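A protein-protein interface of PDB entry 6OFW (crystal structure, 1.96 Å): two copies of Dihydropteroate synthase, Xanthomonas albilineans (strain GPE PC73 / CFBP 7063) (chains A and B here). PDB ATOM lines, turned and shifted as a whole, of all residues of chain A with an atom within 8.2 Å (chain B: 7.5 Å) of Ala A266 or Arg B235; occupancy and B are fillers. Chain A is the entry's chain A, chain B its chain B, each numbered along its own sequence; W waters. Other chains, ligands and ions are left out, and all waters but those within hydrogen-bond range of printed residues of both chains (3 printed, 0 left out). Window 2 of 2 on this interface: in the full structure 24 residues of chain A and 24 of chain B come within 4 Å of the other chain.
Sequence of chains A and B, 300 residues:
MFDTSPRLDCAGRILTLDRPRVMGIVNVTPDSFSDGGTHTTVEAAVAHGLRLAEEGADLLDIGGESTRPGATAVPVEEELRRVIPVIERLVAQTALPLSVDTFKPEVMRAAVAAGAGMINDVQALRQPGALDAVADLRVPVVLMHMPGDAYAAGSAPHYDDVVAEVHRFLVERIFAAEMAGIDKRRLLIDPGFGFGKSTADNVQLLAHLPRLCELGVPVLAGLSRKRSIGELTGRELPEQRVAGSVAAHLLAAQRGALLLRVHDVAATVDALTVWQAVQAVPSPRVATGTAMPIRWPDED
OE1 of Glu A55 lies within hydrogen-bond range of N of Ala A266 (3.0 Å).
The backbone carbonyl oxygen of Val A269 lies within hydrogen-bond range of the side-chain hydroxyl of Thr A273, at 2.7 Å.
O of Ile B229 lies within hydrogen-bond range of OG1 of Thr B233 (2.8 Å).
The backbone carbonyl oxygen (O) of Gly B230 is in hydrogen-bond range of the backbone NH (N) of Arg B235, at 2.9 Å.
The backbone carbonyl oxygen (O) of Arg B235 sits at hydrogen-bond distance from the guanidinium group (NE) of Arg B241, at 3.0 Å.
Printed residues of chain A that touch a printed residue of chain B: Ala A266, Ala A267, Asp A270 and Thr A273.
Hydrophobic or aromatic side chains of chain B within 4 Å of the printed part of chain A: Ala B243.
Among the printed residues, 5 pairs touch across the chains.
The guanidinium group (NE) of Arg B235 is in salt-bridge range of the side-chain carboxylate (OD2) of Asp A270, at 2.8 Å.
Among the printed residues, pairs that only touch across the chains: Thr A273 with Leu B232, Ala A267 with Ala B243, Ala A266 with Arg B235 and Asp A270 with Thr B233.
1 position is printed for both chains.
Of the 5 pairs that touch across the chains among the printed residues, none has its exchanged pair printed and touching as well.
Water W1 bridges the backbone carbonyl oxygen (O) of Glu A55 (2.7 Å) and the guanidinium group (NH2) of Arg B235 (2.8 Å).
Water W3 lies within hydrogen-bond range of the side-chain carboxylate (OD2) of Asp A270 (2.7 Å), the backbone NH (N) of Gly B244 (2.8 Å), the backbone carbonyl oxygen (O) of Gln B240 (3.0 Å) and the backbone NH (N) of Ala B243 (3.2 Å).
Water W2 bridges the side-chain carboxylate (OD1) of Asp A270 and the backbone carbonyl oxygen (O) of Thr B233.
Of chain B, only Arg B235 (3.6 Å) comes within 4 Å of Ala A266.
Arg B235 touches just these residues of chain A: Ala A266 (3.6 Å) and Asp A270 (2.8 Å).
Printed residues of chain B within 4 Å of Thr A273: Leu B232.
Of the printed residues of chain B, Ala A267 touches Ala B243.
Thr A268 touches none of the printed residues of chain B.
The nearest residue of chain A that does not touch Arg B235 is Glu A55 (4.9 Å).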
ATOM      1  N   VAL A  22      26.169  -9.770  -3.151  1.00  0.00           N
ATOM      2  CA  VAL A  22      26.251  -9.102  -1.828  1.00  0.00           C
ATOM      3  C   VAL A  22      25.512  -9.912  -0.750  1.00  0.00           C
ATOM      4  O   VAL A  22      24.332 -10.140  -0.895  1.00  0.00           O
ATOM      5  CB  VAL A  22      25.782  -7.638  -1.912  1.00  0.00           C
ATOM      6  CG1 VAL A  22      25.700  -6.992  -0.557  1.00  0.00           C
ATOM      7  CG2 VAL A  22      26.642  -6.796  -2.849  1.00  0.00           C
ATOM      8  N   ARG A  51      15.333  -4.769   5.757  1.00  0.00           N
ATOM      9  CA  ARG A  51      15.935  -3.520   5.255  1.00  0.00           C
ATOM     10  C   ARG A  51      17.069  -3.850   4.268  1.00  0.00           C
ATOM     11  O   ARG A  51      17.108  -3.313   3.167  1.00  0.00           O
ATOM     12  CB  ARG A  51      16.473  -2.668   6.413  1.00  0.00           C
ATOM     13  N   LEU A  52      17.943  -4.805   4.636  1.00  0.00           N
ATOM     14  CA  LEU A  52      19.037  -5.228   3.754  1.00  0.00           C
ATOM     15  C   LEU A  52      18.521  -5.857   2.442  1.00  0.00           C
ATOM     16  O   LEU A  52      19.114  -5.639   1.388  1.00  0.00           O
ATOM     17  CB  LEU A  52      20.006  -6.161   4.502  1.00  0.00           C
ATOM     18  CG  LEU A  52      20.727  -5.555   5.730  1.00  0.00           C
ATOM     19  CD1 LEU A  52      21.877  -6.444   6.156  1.00  0.00           C
ATOM     20  CD2 LEU A  52      21.237  -4.109   5.477  1.00  0.00           C
ATOM     21  N   GLU A  54      15.637  -5.026   0.938  1.00  0.00           N
ATOM     22  CA  GLU A  54      15.185  -3.828   0.211  1.00  0.00           C
ATOM     23  C   GLU A  54      16.377  -3.070  -0.405  1.00  0.00           C
ATOM     24  O   GLU A  54      16.237  -2.503  -1.484  1.00  0.00           O
ATOM     25  CB  GLU A  54      14.412  -2.885   1.151  1.00  0.00           C
ATOM     26  N   GLU A  55      17.560  -3.088   0.273  1.00  0.00           N
ATOM     27  CA  GLU A  55      18.780  -2.419  -0.201  1.00  0.00           C
ATOM     28  C   GLU A  55      19.473  -3.186  -1.343  1.00  0.00           C
ATOM     29  O   GLU A  55      20.432  -2.686  -1.941  1.00  0.00           O
ATOM     30  CB  GLU A  55      19.750  -2.162   0.959  1.00  0.00           C
ATOM     31  CG  GLU A  55      19.286  -1.079   1.908  1.00  0.00           C
ATOM     32  CD  GLU A  55      20.279  -0.746   3.001  1.00  0.00           C
ATOM     33  OE1 GLU A  55      21.444  -1.193   2.906  1.00  0.00           O
ATOM     34  OE2 GLU A  55      19.891  -0.043   3.961  1.00  0.00           O
ATOM     35  N   GLY A  56      18.975  -4.371  -1.664  1.00  0.00           N
ATOM     36  CA  GLY A  56      19.511  -5.134  -2.785  1.00  0.00           C
ATOM     37  C   GLY A  56      20.483  -6.236  -2.417  1.00  0.00           C
ATOM     38  O   GLY A  56      21.254  -6.681  -3.269  1.00  0.00           O
ATOM     39  N   ALA A  57      20.414  -6.742  -1.171  1.00  0.00           N
ATOM     40  CA  ALA A  57      21.255  -7.879  -0.780  1.00  0.00           C
ATOM     41  C   ALA A  57      20.863  -9.076  -1.640  1.00  0.00           C
ATOM     42  O   ALA A  57      19.680  -9.254  -1.939  1.00  0.00           O
ATOM     43  CB  ALA A  57      21.020  -8.218   0.685  1.00  0.00           C
ATOM     44  N   VAL A 242      32.741   2.906   6.879  1.00  0.00           N
ATOM     45  CA  VAL A 242      31.906   2.574   5.705  1.00  0.00           C
ATOM     46  C   VAL A 242      32.597   2.862   4.371  1.00  0.00           C
ATOM     47  O   VAL A 242      32.676   1.971   3.531  1.00  0.00           O
ATOM     48  CB  VAL A 242      30.514   3.229   5.776  1.00  0.00           C
ATOM     49  CG1 VAL A 242      29.677   2.871   4.534  1.00  0.00           C
ATOM     50  CG2 VAL A 242      29.803   2.802   7.061  1.00  0.00           C
ATOM     51  N   VAL A 246      33.554  -0.060   1.706  1.00  0.00           N
ATOM     52  CA  VAL A 246      32.931  -0.102   0.358  1.00  0.00           C
ATOM     53  C   VAL A 246      34.066  -0.165  -0.686  1.00  0.00           C
ATOM     54  O   VAL A 246      34.016  -0.990  -1.598  1.00  0.00           O
ATOM     55  CB  VAL A 246      31.962   1.104   0.133  1.00  0.00           C
ATOM     56  CG1 VAL A 246      31.493   1.177  -1.325  1.00  0.00           C
ATOM     57  CG2 VAL A 246      30.751   1.024   1.063  1.00  0.00           C
ATOM     58  N   VAL A 262      28.912  -7.849   3.814  1.00  0.00           N
ATOM     59  CA  VAL A 262      28.893  -6.436   4.192  1.00  0.00           C
ATOM     60  C   VAL A 262      27.748  -6.023   5.116  1.00  0.00           C
ATOM     61  O   VAL A 262      26.684  -6.623   5.094  1.00  0.00           O
ATOM     62  CB  VAL A 262      28.923  -5.524   2.915  1.00  0.00           C
ATOM     63  CG1 VAL A 262      29.960  -6.003   1.890  1.00  0.00           C
ATOM     64  CG2 VAL A 262      27.548  -5.424   2.245  1.00  0.00           C
ATOM     65  N   HIS A 263      27.975  -4.964   5.898  1.00  0.00           N
ATOM     66  CA  HIS A 263      26.922  -4.349   6.718  1.00  0.00           C
ATOM     67  C   HIS A 263      26.194  -3.327   5.821  1.00  0.00           C
ATOM     68  O   HIS A 263      24.972  -3.192   5.890  1.00  0.00           O
ATOM     69  CB  HIS A 263      27.543  -3.589   7.913  1.00  0.00           C
ATOM     70  CG  HIS A 263      28.251  -4.467   8.906  1.00  0.00           C
ATOM     71  ND1 HIS A 263      29.631  -4.629   8.886  1.00  0.00           N
ATOM     72  CD2 HIS A 263      27.742  -5.189   9.935  1.00  0.00           C
ATOM     73  CE1 HIS A 263      29.914  -5.444   9.893  1.00  0.00           C
ATOM     74  NE2 HIS A 263      28.810  -5.793  10.561  1.00  0.00           N
ATOM     75  N   ASP A 264      26.967  -2.613   4.961  1.00  0.00           N
ATOM     76  CA  ASP A 264      26.523  -1.501   4.147  1.00  0.00           C
ATOM     77  C   ASP A 264      26.110  -1.951   2.767  1.00  0.00           C
ATOM     78  O   ASP A 264      26.826  -1.780   1.763  1.00  0.00           O
ATOM     79  CB  ASP A 264      27.591  -0.391   4.159  1.00  0.00           C
ATOM     80  CG  ASP A 264      27.942  -0.034   5.598  1.00  0.00           C
ATOM     81  OD1 ASP A 264      27.157   0.731   6.241  1.00  0.00           O
ATOM     82  OD2 ASP A 264      28.943  -0.547   6.094  1.00  0.00           O
ATOM     83  N   VAL A 265      24.930  -2.543   2.727  1.00  0.00           N
ATOM     84  CA  VAL A 265      24.408  -3.165   1.504  1.00  0.00           C
ATOM     85  C   VAL A 265      24.157  -2.167   0.391  1.00  0.00           C
ATOM     86  O   VAL A 265      24.705  -2.375  -0.694  1.00  0.00           O
ATOM     87  CB  VAL A 265      23.184  -4.058   1.773  1.00  0.00           C
ATOM     88  CG1 VAL A 265      22.583  -4.575   0.456  1.00  0.00           C
ATOM     89  CG2 VAL A 265      23.573  -5.239   2.680  1.00  0.00           C
ATOM     90  N   ALA A 266      23.326  -1.124   0.613  1.00  0.00           N
ATOM     91  CA  ALA A 266      22.976  -0.171  -0.477  1.00  0.00           C
ATOM     92  C   ALA A 266      24.204   0.496  -1.039  1.00  0.00           C
ATOM     93  O   ALA A 266      24.338   0.609  -2.262  1.00  0.00           O
ATOM     94  CB  ALA A 266      21.981   0.894   0.022  1.00  0.00           C
ATOM     95  N   ALA A 267      25.156   0.846  -0.153  1.00  0.00           N
ATOM     96  CA  ALA A 267      26.386   1.513  -0.572  1.00  0.00           C
ATOM     97  C   ALA A 267      27.269   0.587  -1.410  1.00  0.00           C
ATOM     98  O   ALA A 267      27.807   1.022  -2.426  1.00  0.00           O
ATOM     99  CB  ALA A 267      27.137   2.035   0.653  1.00  0.00           C
ATOM    100  N   THR A 268      27.402  -0.690  -1.004  1.00  0.00           N
ATOM    101  CA  THR A 268      28.226  -1.677  -1.740  1.00  0.00           C
ATOM    102  C   THR A 268      27.536  -1.974  -3.095  1.00  0.00           C
ATOM    103  O   THR A 268      28.200  -2.095  -4.126  1.00  0.00           O
ATOM    104  CB  THR A 268      28.437  -2.946  -0.881  1.00  0.00           C
ATOM    105  OG1 THR A 268      29.004  -2.553   0.383  1.00  0.00           O
ATOM    106  CG2 THR A 268      29.345  -3.991  -1.581  1.00  0.00           C
ATOM    107  N   VAL A 269      26.206  -2.112  -3.082  1.00  0.00           N
ATOM    108  CA  VAL A 269      25.451  -2.323  -4.332  1.00  0.00           C
ATOM    109  C   VAL A 269      25.766  -1.162  -5.326  1.00  0.00           C
ATOM    110  O   VAL A 269      26.138  -1.421  -6.469  1.00  0.00           O
ATOM    111  CB  VAL A 269      23.931  -2.543  -4.074  1.00  0.00           C
ATOM    112  CG1 VAL A 269      23.105  -2.432  -5.373  1.00  0.00           C
ATOM    113  CG2 VAL A 269      23.694  -3.911  -3.400  1.00  0.00           C
ATOM    114  N   ASP A 270      25.655   0.096  -4.882  1.00  0.00           N
ATOM    115  CA  ASP A 270      25.938   1.261  -5.743  1.00  0.00           C
ATOM    116  C   ASP A 270      27.361   1.239  -6.304  1.00  0.00           C
ATOM    117  O   ASP A 270      27.543   1.503  -7.496  1.00  0.00           O
ATOM    118  CB  ASP A 270      25.691   2.555  -4.980  1.00  0.00           C
ATOM    119  CG  ASP A 270      24.238   2.827  -4.685  1.00  0.00           C
ATOM    120  OD1 ASP A 270      23.393   1.953  -5.001  1.00  0.00           O
ATOM    121  OD2 ASP A 270      23.945   3.901  -4.112  1.00  0.00           O
ATOM    122  N   ALA A 271      28.371   0.917  -5.459  1.00  0.00           N
ATOM    123  CA  ALA A 271      29.766   0.833  -5.911  1.00  0.00           C
ATOM    124  C   ALA A 271      29.940  -0.216  -6.999  1.00  0.00           C
ATOM    125  O   ALA A 271      30.566   0.060  -8.020  1.00  0.00           O
ATOM    126  CB  ALA A 271      30.701   0.533  -4.732  1.00  0.00           C
ATOM    127  N   LEU A 272      29.397  -1.414  -6.784  1.00  0.00           N
ATOM    128  CA  LEU A 272      29.508  -2.509  -7.760  1.00  0.00           C
ATOM    129  C   LEU A 272      28.744  -2.216  -9.056  1.00  0.00           C
ATOM    130  O   LEU A 272      29.181  -2.630 -10.126  1.00  0.00           O
ATOM    131  CB  LEU A 272      28.964  -3.821  -7.155  1.00  0.00           C
ATOM    132  CG  LEU A 272      29.701  -4.388  -5.949  1.00  0.00           C
ATOM    133  CD1 LEU A 272      28.840  -5.455  -5.272  1.00  0.00           C
ATOM    134  CD2 LEU A 272      31.095  -4.933  -6.344  1.00  0.00           C
ATOM    135  N   THR A 273      27.612  -1.527  -8.959  1.00  0.00           N
ATOM    136  CA  THR A 273      26.796  -1.156 -10.132  1.00  0.00           C
ATOM    137  C   THR A 273      27.592  -0.199 -11.050  1.00  0.00           C
ATOM    138  O   THR A 273      27.666  -0.429 -12.261  1.00  0.00           O
ATOM    139  CB  THR A 273      25.454  -0.582  -9.675  1.00  0.00           C
ATOM    140  OG1 THR A 273      24.820  -1.561  -8.862  1.00  0.00           O
ATOM    141  CG2 THR A 273      24.538  -0.233 -10.836  1.00  0.00           C
ATOM    142  N   ARG B 225      28.425  13.302  -7.463  1.00  0.00           N
ATOM    143  CA  ARG B 225      26.965  13.332  -7.263  1.00  0.00           C
ATOM    144  C   ARG B 225      26.214  13.728  -8.530  1.00  0.00           C
ATOM    145  O   ARG B 225      25.108  14.265  -8.452  1.00  0.00           O
ATOM    146  CB  ARG B 225      26.604  14.312  -6.136  1.00  0.00           C
ATOM    147  CG  ARG B 225      27.286  14.028  -4.798  1.00  0.00           C
ATOM    148  CD  ARG B 225      26.838  15.077  -3.822  1.00  0.00           C
ATOM    149  NE  ARG B 225      27.359  14.810  -2.485  1.00  0.00           N
ATOM    150  CZ  ARG B 225      27.010  15.509  -1.421  1.00  0.00           C
ATOM    151  NH1 ARG B 225      26.143  16.511  -1.528  1.00  0.00           N
ATOM    152  NH2 ARG B 225      27.518  15.213  -0.236  1.00  0.00           N
ATOM    153  N   LYS B 226      26.828  13.492  -9.681  1.00  0.00           N
ATOM    154  CA  LYS B 226      26.290  13.901 -10.961  1.00  0.00           C
ATOM    155  C   LYS B 226      25.123  13.018 -11.398  1.00  0.00           C
ATOM    156  O   LYS B 226      24.970  11.890 -10.927  1.00  0.00           O
ATOM    157  CB  LYS B 226      27.425  13.993 -12.009  1.00  0.00           C
ATOM    158  CG  LYS B 226      28.251  15.283 -11.817  1.00  0.00           C
ATOM    159  CD  LYS B 226      29.268  15.536 -12.912  1.00  0.00           C
ATOM    160  CE  LYS B 226      29.969  16.845 -12.648  1.00  0.00           C
ATOM    161  NZ  LYS B 226      31.071  17.113 -13.611  1.00  0.00           N
ATOM    162  N   ARG B 227      24.255  13.573 -12.257  1.00  0.00           N
ATOM    163  CA  ARG B 227      23.066  12.867 -12.732  1.00  0.00           C
ATOM    164  C   ARG B 227      23.388  11.483 -13.319  1.00  0.00           C
ATOM    165  O   ARG B 227      22.641  10.562 -13.061  1.00  0.00           O
ATOM    166  CB  ARG B 227      22.291  13.755 -13.708  1.00  0.00           C
ATOM    167  CG  ARG B 227      20.998  13.135 -14.250  1.00  0.00           C
ATOM    168  CD  ARG B 227      20.441  13.931 -15.415  1.00  0.00           C
ATOM    169  NE  ARG B 227      19.688  15.103 -14.963  1.00  0.00           N
ATOM    170  CZ  ARG B 227      20.155  16.348 -14.961  1.00  0.00           C
ATOM    171  NH1 ARG B 227      21.382  16.608 -15.399  1.00  0.00           N
ATOM    172  NH2 ARG B 227      19.394  17.346 -14.530  1.00  0.00           N
ATOM    173  N   ILE B 229      25.667   9.403 -12.374  1.00  0.00           N
ATOM    174  CA  ILE B 229      25.875   8.501 -11.234  1.00  0.00           C
ATOM    175  C   ILE B 229      24.504   8.084 -10.713  1.00  0.00           C
ATOM    176  O   ILE B 229      24.261   6.898 -10.476  1.00  0.00           O
ATOM    177  CB  ILE B 229      26.783   9.115 -10.125  1.00  0.00           C
ATOM    178  CG1 ILE B 229      28.205   9.408 -10.654  1.00  0.00           C
ATOM    179  CG2 ILE B 229      26.843   8.195  -8.884  1.00  0.00           C
ATOM    180  CD1 ILE B 229      28.958   8.203 -11.396  1.00  0.00           C
ATOM    181  N   GLY B 230      23.610   9.070 -10.616  1.00  0.00           N
ATOM    182  CA  GLY B 230      22.224   8.885 -10.204  1.00  0.00           C
ATOM    183  C   GLY B 230      21.501   7.910 -11.109  1.00  0.00           C
ATOM    184  O   GLY B 230      20.801   7.040 -10.615  1.00  0.00           O
ATOM    185  N   GLU B 231      21.721   7.997 -12.431  1.00  0.00           N
ATOM    186  CA  GLU B 231      21.102   7.083 -13.419  1.00  0.00           C
ATOM    187  C   GLU B 231      21.656   5.658 -13.295  1.00  0.00           C
ATOM    188  O   GLU B 231      20.890   4.706 -13.356  1.00  0.00           O
ATOM    189  CB  GLU B 231      21.304   7.600 -14.862  1.00  0.00           C
ATOM    190  CG  GLU B 231      20.497   8.854 -15.192  1.00  0.00           C
ATOM    191  CD  GLU B 231      18.978   8.820 -15.098  1.00  0.00           C
ATOM    192  OE1 GLU B 231      18.383   7.716 -15.149  1.00  0.00           O
ATOM    193  OE2 GLU B 231      18.376   9.913 -14.988  1.00  0.00           O
ATOM    194  N   LEU B 232      22.983   5.518 -13.097  1.00  0.00           N
ATOM    195  CA  LEU B 232      23.608   4.202 -12.970  1.00  0.00           C
ATOM    196  C   LEU B 232      23.164   3.462 -11.728  1.00  0.00           C
ATOM    197  O   LEU B 232      23.031   2.244 -11.773  1.00  0.00           O
ATOM    198  CB  LEU B 232      25.137   4.310 -12.947  1.00  0.00           C
ATOM    199  CG  LEU B 232      25.840   4.717 -14.229  1.00  0.00           C
ATOM    200  CD1 LEU B 232      27.339   4.799 -13.999  1.00  0.00           C
ATOM    201  CD2 LEU B 232      25.510   3.763 -15.377  1.00  0.00           C
ATOM    202  N   THR B 233      22.896   4.193 -10.625  1.00  0.00           N
ATOM    203  CA  THR B 233      22.558   3.579  -9.344  1.00  0.00           C
ATOM    204  C   THR B 233      21.092   3.672  -8.933  1.00  0.00           C
ATOM    205  O   THR B 233      20.725   3.085  -7.913  1.00  0.00           O
ATOM    206  CB  THR B 233      23.422   4.214  -8.243  1.00  0.00           C
ATOM    207  OG1 THR B 233      23.150   5.615  -8.232  1.00  0.00           O
ATOM    208  CG2 THR B 233      24.910   3.971  -8.445  1.00  0.00           C
ATOM    209  N   GLY B 234      20.301   4.447  -9.680  1.00  0.00           N
ATOM    210  CA  GLY B 234      18.906   4.694  -9.358  1.00  0.00           C
ATOM    211  C   GLY B 234      18.744   5.608  -8.165  1.00  0.00           C
ATOM    212  O   GLY B 234      17.742   5.518  -7.458  1.00  0.00           O
ATOM    213  N   ARG B 235      19.719   6.518  -7.935  1.00  0.00           N
ATOM    214  CA  ARG B 235      19.685   7.437  -6.784  1.00  0.00           C
ATOM    215  C   ARG B 235      19.257   8.808  -7.274  1.00  0.00           C
ATOM    216  O   ARG B 235      20.021   9.496  -7.944  1.00  0.00           O
ATOM    217  CB  ARG B 235      21.052   7.488  -6.057  1.00  0.00           C
ATOM    218  CG  ARG B 235      21.550   6.137  -5.533  1.00  0.00           C
ATOM    219  CD  ARG B 235      20.672   5.484  -4.472  1.00  0.00           C
ATOM    220  NE  ARG B 235      21.181   4.148  -4.166  1.00  0.00           N
ATOM    221  CZ  ARG B 235      20.511   3.183  -3.547  1.00  0.00           C
ATOM    222  NH1 ARG B 235      19.247   3.367  -3.183  1.00  0.00           N
ATOM    223  NH2 ARG B 235      21.089   2.013  -3.321  1.00  0.00           N
ATOM    224  N   GLU B 236      18.028   9.206  -6.942  1.00  0.00           N
ATOM    225  CA  GLU B 236      17.440  10.456  -7.432  1.00  0.00           C
ATOM    226  C   GLU B 236      18.023  11.732  -6.857  1.00  0.00           C
ATOM    227  O   GLU B 236      18.084  12.720  -7.573  1.00  0.00           O
ATOM    228  CB  GLU B 236      15.922  10.448  -7.232  1.00  0.00           C
ATOM    229  N   LEU B 237      18.415  11.735  -5.589  1.00  0.00           N
ATOM    230  CA  LEU B 237      18.920  12.961  -4.962  1.00  0.00           C
ATOM    231  C   LEU B 237      20.450  13.023  -4.894  1.00  0.00           C
ATOM    232  O   LEU B 237      21.059  11.980  -4.680  1.00  0.00           O
ATOM    233  CB  LEU B 237      18.284  13.149  -3.578  1.00  0.00           C
ATOM    234  CG  LEU B 237      16.733  13.112  -3.515  1.00  0.00           C
ATOM    235  CD1 LEU B 237      16.254  13.188  -2.076  1.00  0.00           C
ATOM    236  CD2 LEU B 237      16.105  14.258  -4.331  1.00  0.00           C
ATOM    237  N   PRO B 238      21.081  14.216  -5.093  1.00  0.00           N
ATOM    238  CA  PRO B 238      22.560  14.287  -5.075  1.00  0.00           C
ATOM    239  C   PRO B 238      23.206  13.634  -3.876  1.00  0.00           C
ATOM    240  O   PRO B 238      24.149  12.868  -4.042  1.00  0.00           O
ATOM    241  CB  PRO B 238      22.852  15.792  -5.138  1.00  0.00           C
ATOM    242  CG  PRO B 238      21.666  16.366  -5.843  1.00  0.00           C
ATOM    243  CD  PRO B 238      20.484  15.547  -5.370  1.00  0.00           C
ATOM    244  N   GLU B 239      22.635  13.895  -2.695  1.00  0.00           N
ATOM    245  CA  GLU B 239      23.152  13.406  -1.427  1.00  0.00           C
ATOM    246  C   GLU B 239      23.034  11.876  -1.254  1.00  0.00           C
ATOM    247  O   GLU B 239      23.654  11.355  -0.347  1.00  0.00           O
ATOM    248  CB  GLU B 239      22.536  14.171  -0.230  1.00  0.00           C
ATOM    249  CG  GLU B 239      21.042  13.941  -0.031  1.00  0.00           C
ATOM    250  CD  GLU B 239      20.117  14.898  -0.763  1.00  0.00           C
ATOM    251  OE1 GLU B 239      18.911  14.911  -0.423  1.00  0.00           O
ATOM    252  OE2 GLU B 239      20.584  15.631  -1.666  1.00  0.00           O
ATOM    253  N   GLN B 240      22.277  11.174  -2.126  1.00  0.00           N
ATOM    254  CA  GLN B 240      22.111   9.709  -2.131  1.00  0.00           C
ATOM    255  C   GLN B 240      23.141   9.066  -3.071  1.00  0.00           C
ATOM    256  O   GLN B 240      23.240   7.854  -3.126  1.00  0.00           O
ATOM    257  CB  GLN B 240      20.702   9.336  -2.627  1.00  0.00           C
ATOM    258  CG  GLN B 240      19.555   9.737  -1.696  1.00  0.00           C
ATOM    259  CD  GLN B 240      18.198   9.534  -2.361  1.00  0.00           C
ATOM    260  OE1 GLN B 240      18.073   9.429  -3.586  1.00  0.00           O
ATOM    261  NE2 GLN B 240      17.149   9.466  -1.562  1.00  0.00           N
ATOM    262  N   ARG B 241      23.891   9.896  -3.827  1.00  0.00           N
ATOM    263  CA  ARG B 241      24.870   9.432  -4.822  1.00  0.00           C
ATOM    264  C   ARG B 241      26.318   9.343  -4.301  1.00  0.00           C
ATOM    265  O   ARG B 241      27.239   9.163  -5.096  1.00  0.00           O
ATOM    266  CB  ARG B 241      24.826  10.353  -6.063  1.00  0.00           C
ATOM    267  CG  ARG B 241      23.463  10.372  -6.770  1.00  0.00           C
ATOM    268  CD  ARG B 241      23.369  11.519  -7.740  1.00  0.00           C
ATOM    269  NE  ARG B 241      22.012  11.653  -8.279  1.00  0.00           N
ATOM    270  CZ  ARG B 241      21.569  12.703  -8.956  1.00  0.00           C
ATOM    271  NH1 ARG B 241      22.362  13.743  -9.172  1.00  0.00           N
ATOM    272  NH2 ARG B 241      20.320  12.729  -9.407  1.00  0.00           N
ATOM    273  N   VAL B 242      26.528   9.415  -2.996  1.00  0.00           N
ATOM    274  CA  VAL B 242      27.899   9.398  -2.423  1.00  0.00           C
ATOM    275  C   VAL B 242      28.668   8.097  -2.725  1.00  0.00           C
ATOM    276  O   VAL B 242      29.770   8.167  -3.279  1.00  0.00           O
ATOM    277  CB  VAL B 242      27.923   9.734  -0.930  1.00  0.00           C
ATOM    278  CG1 VAL B 242      29.368   9.720  -0.388  1.00  0.00           C
ATOM    279  CG2 VAL B 242      27.258  11.099  -0.676  1.00  0.00           C
ATOM    280  N   ALA B 243      28.089   6.929  -2.405  1.00  0.00           N
ATOM    281  CA  ALA B 243      28.765   5.662  -2.672  1.00  0.00           C
ATOM    282  C   ALA B 243      29.097   5.505  -4.140  1.00  0.00           C
ATOM    283  O   ALA B 243      30.219   5.140  -4.465  1.00  0.00           O
ATOM    284  CB  ALA B 243      27.928   4.486  -2.192  1.00  0.00           C
ATOM    285  N   GLY B 244      28.147   5.810  -5.036  1.00  0.00           N
ATOM    286  CA  GLY B 244      28.412   5.675  -6.466  1.00  0.00           C
ATOM    287  C   GLY B 244      29.478   6.642  -6.959  1.00  0.00           C
ATOM    288  O   GLY B 244      30.249   6.311  -7.865  1.00  0.00           O
HETATM  289  O   HOH W   1      19.687  -0.426  -3.144  1.00  0.00           O
HETATM  290  O   HOH W   2      21.868   0.716  -6.949  1.00  0.00           O
HETATM  291  O   HOH W   3      25.501   6.104  -4.163  1.00  0.00           O
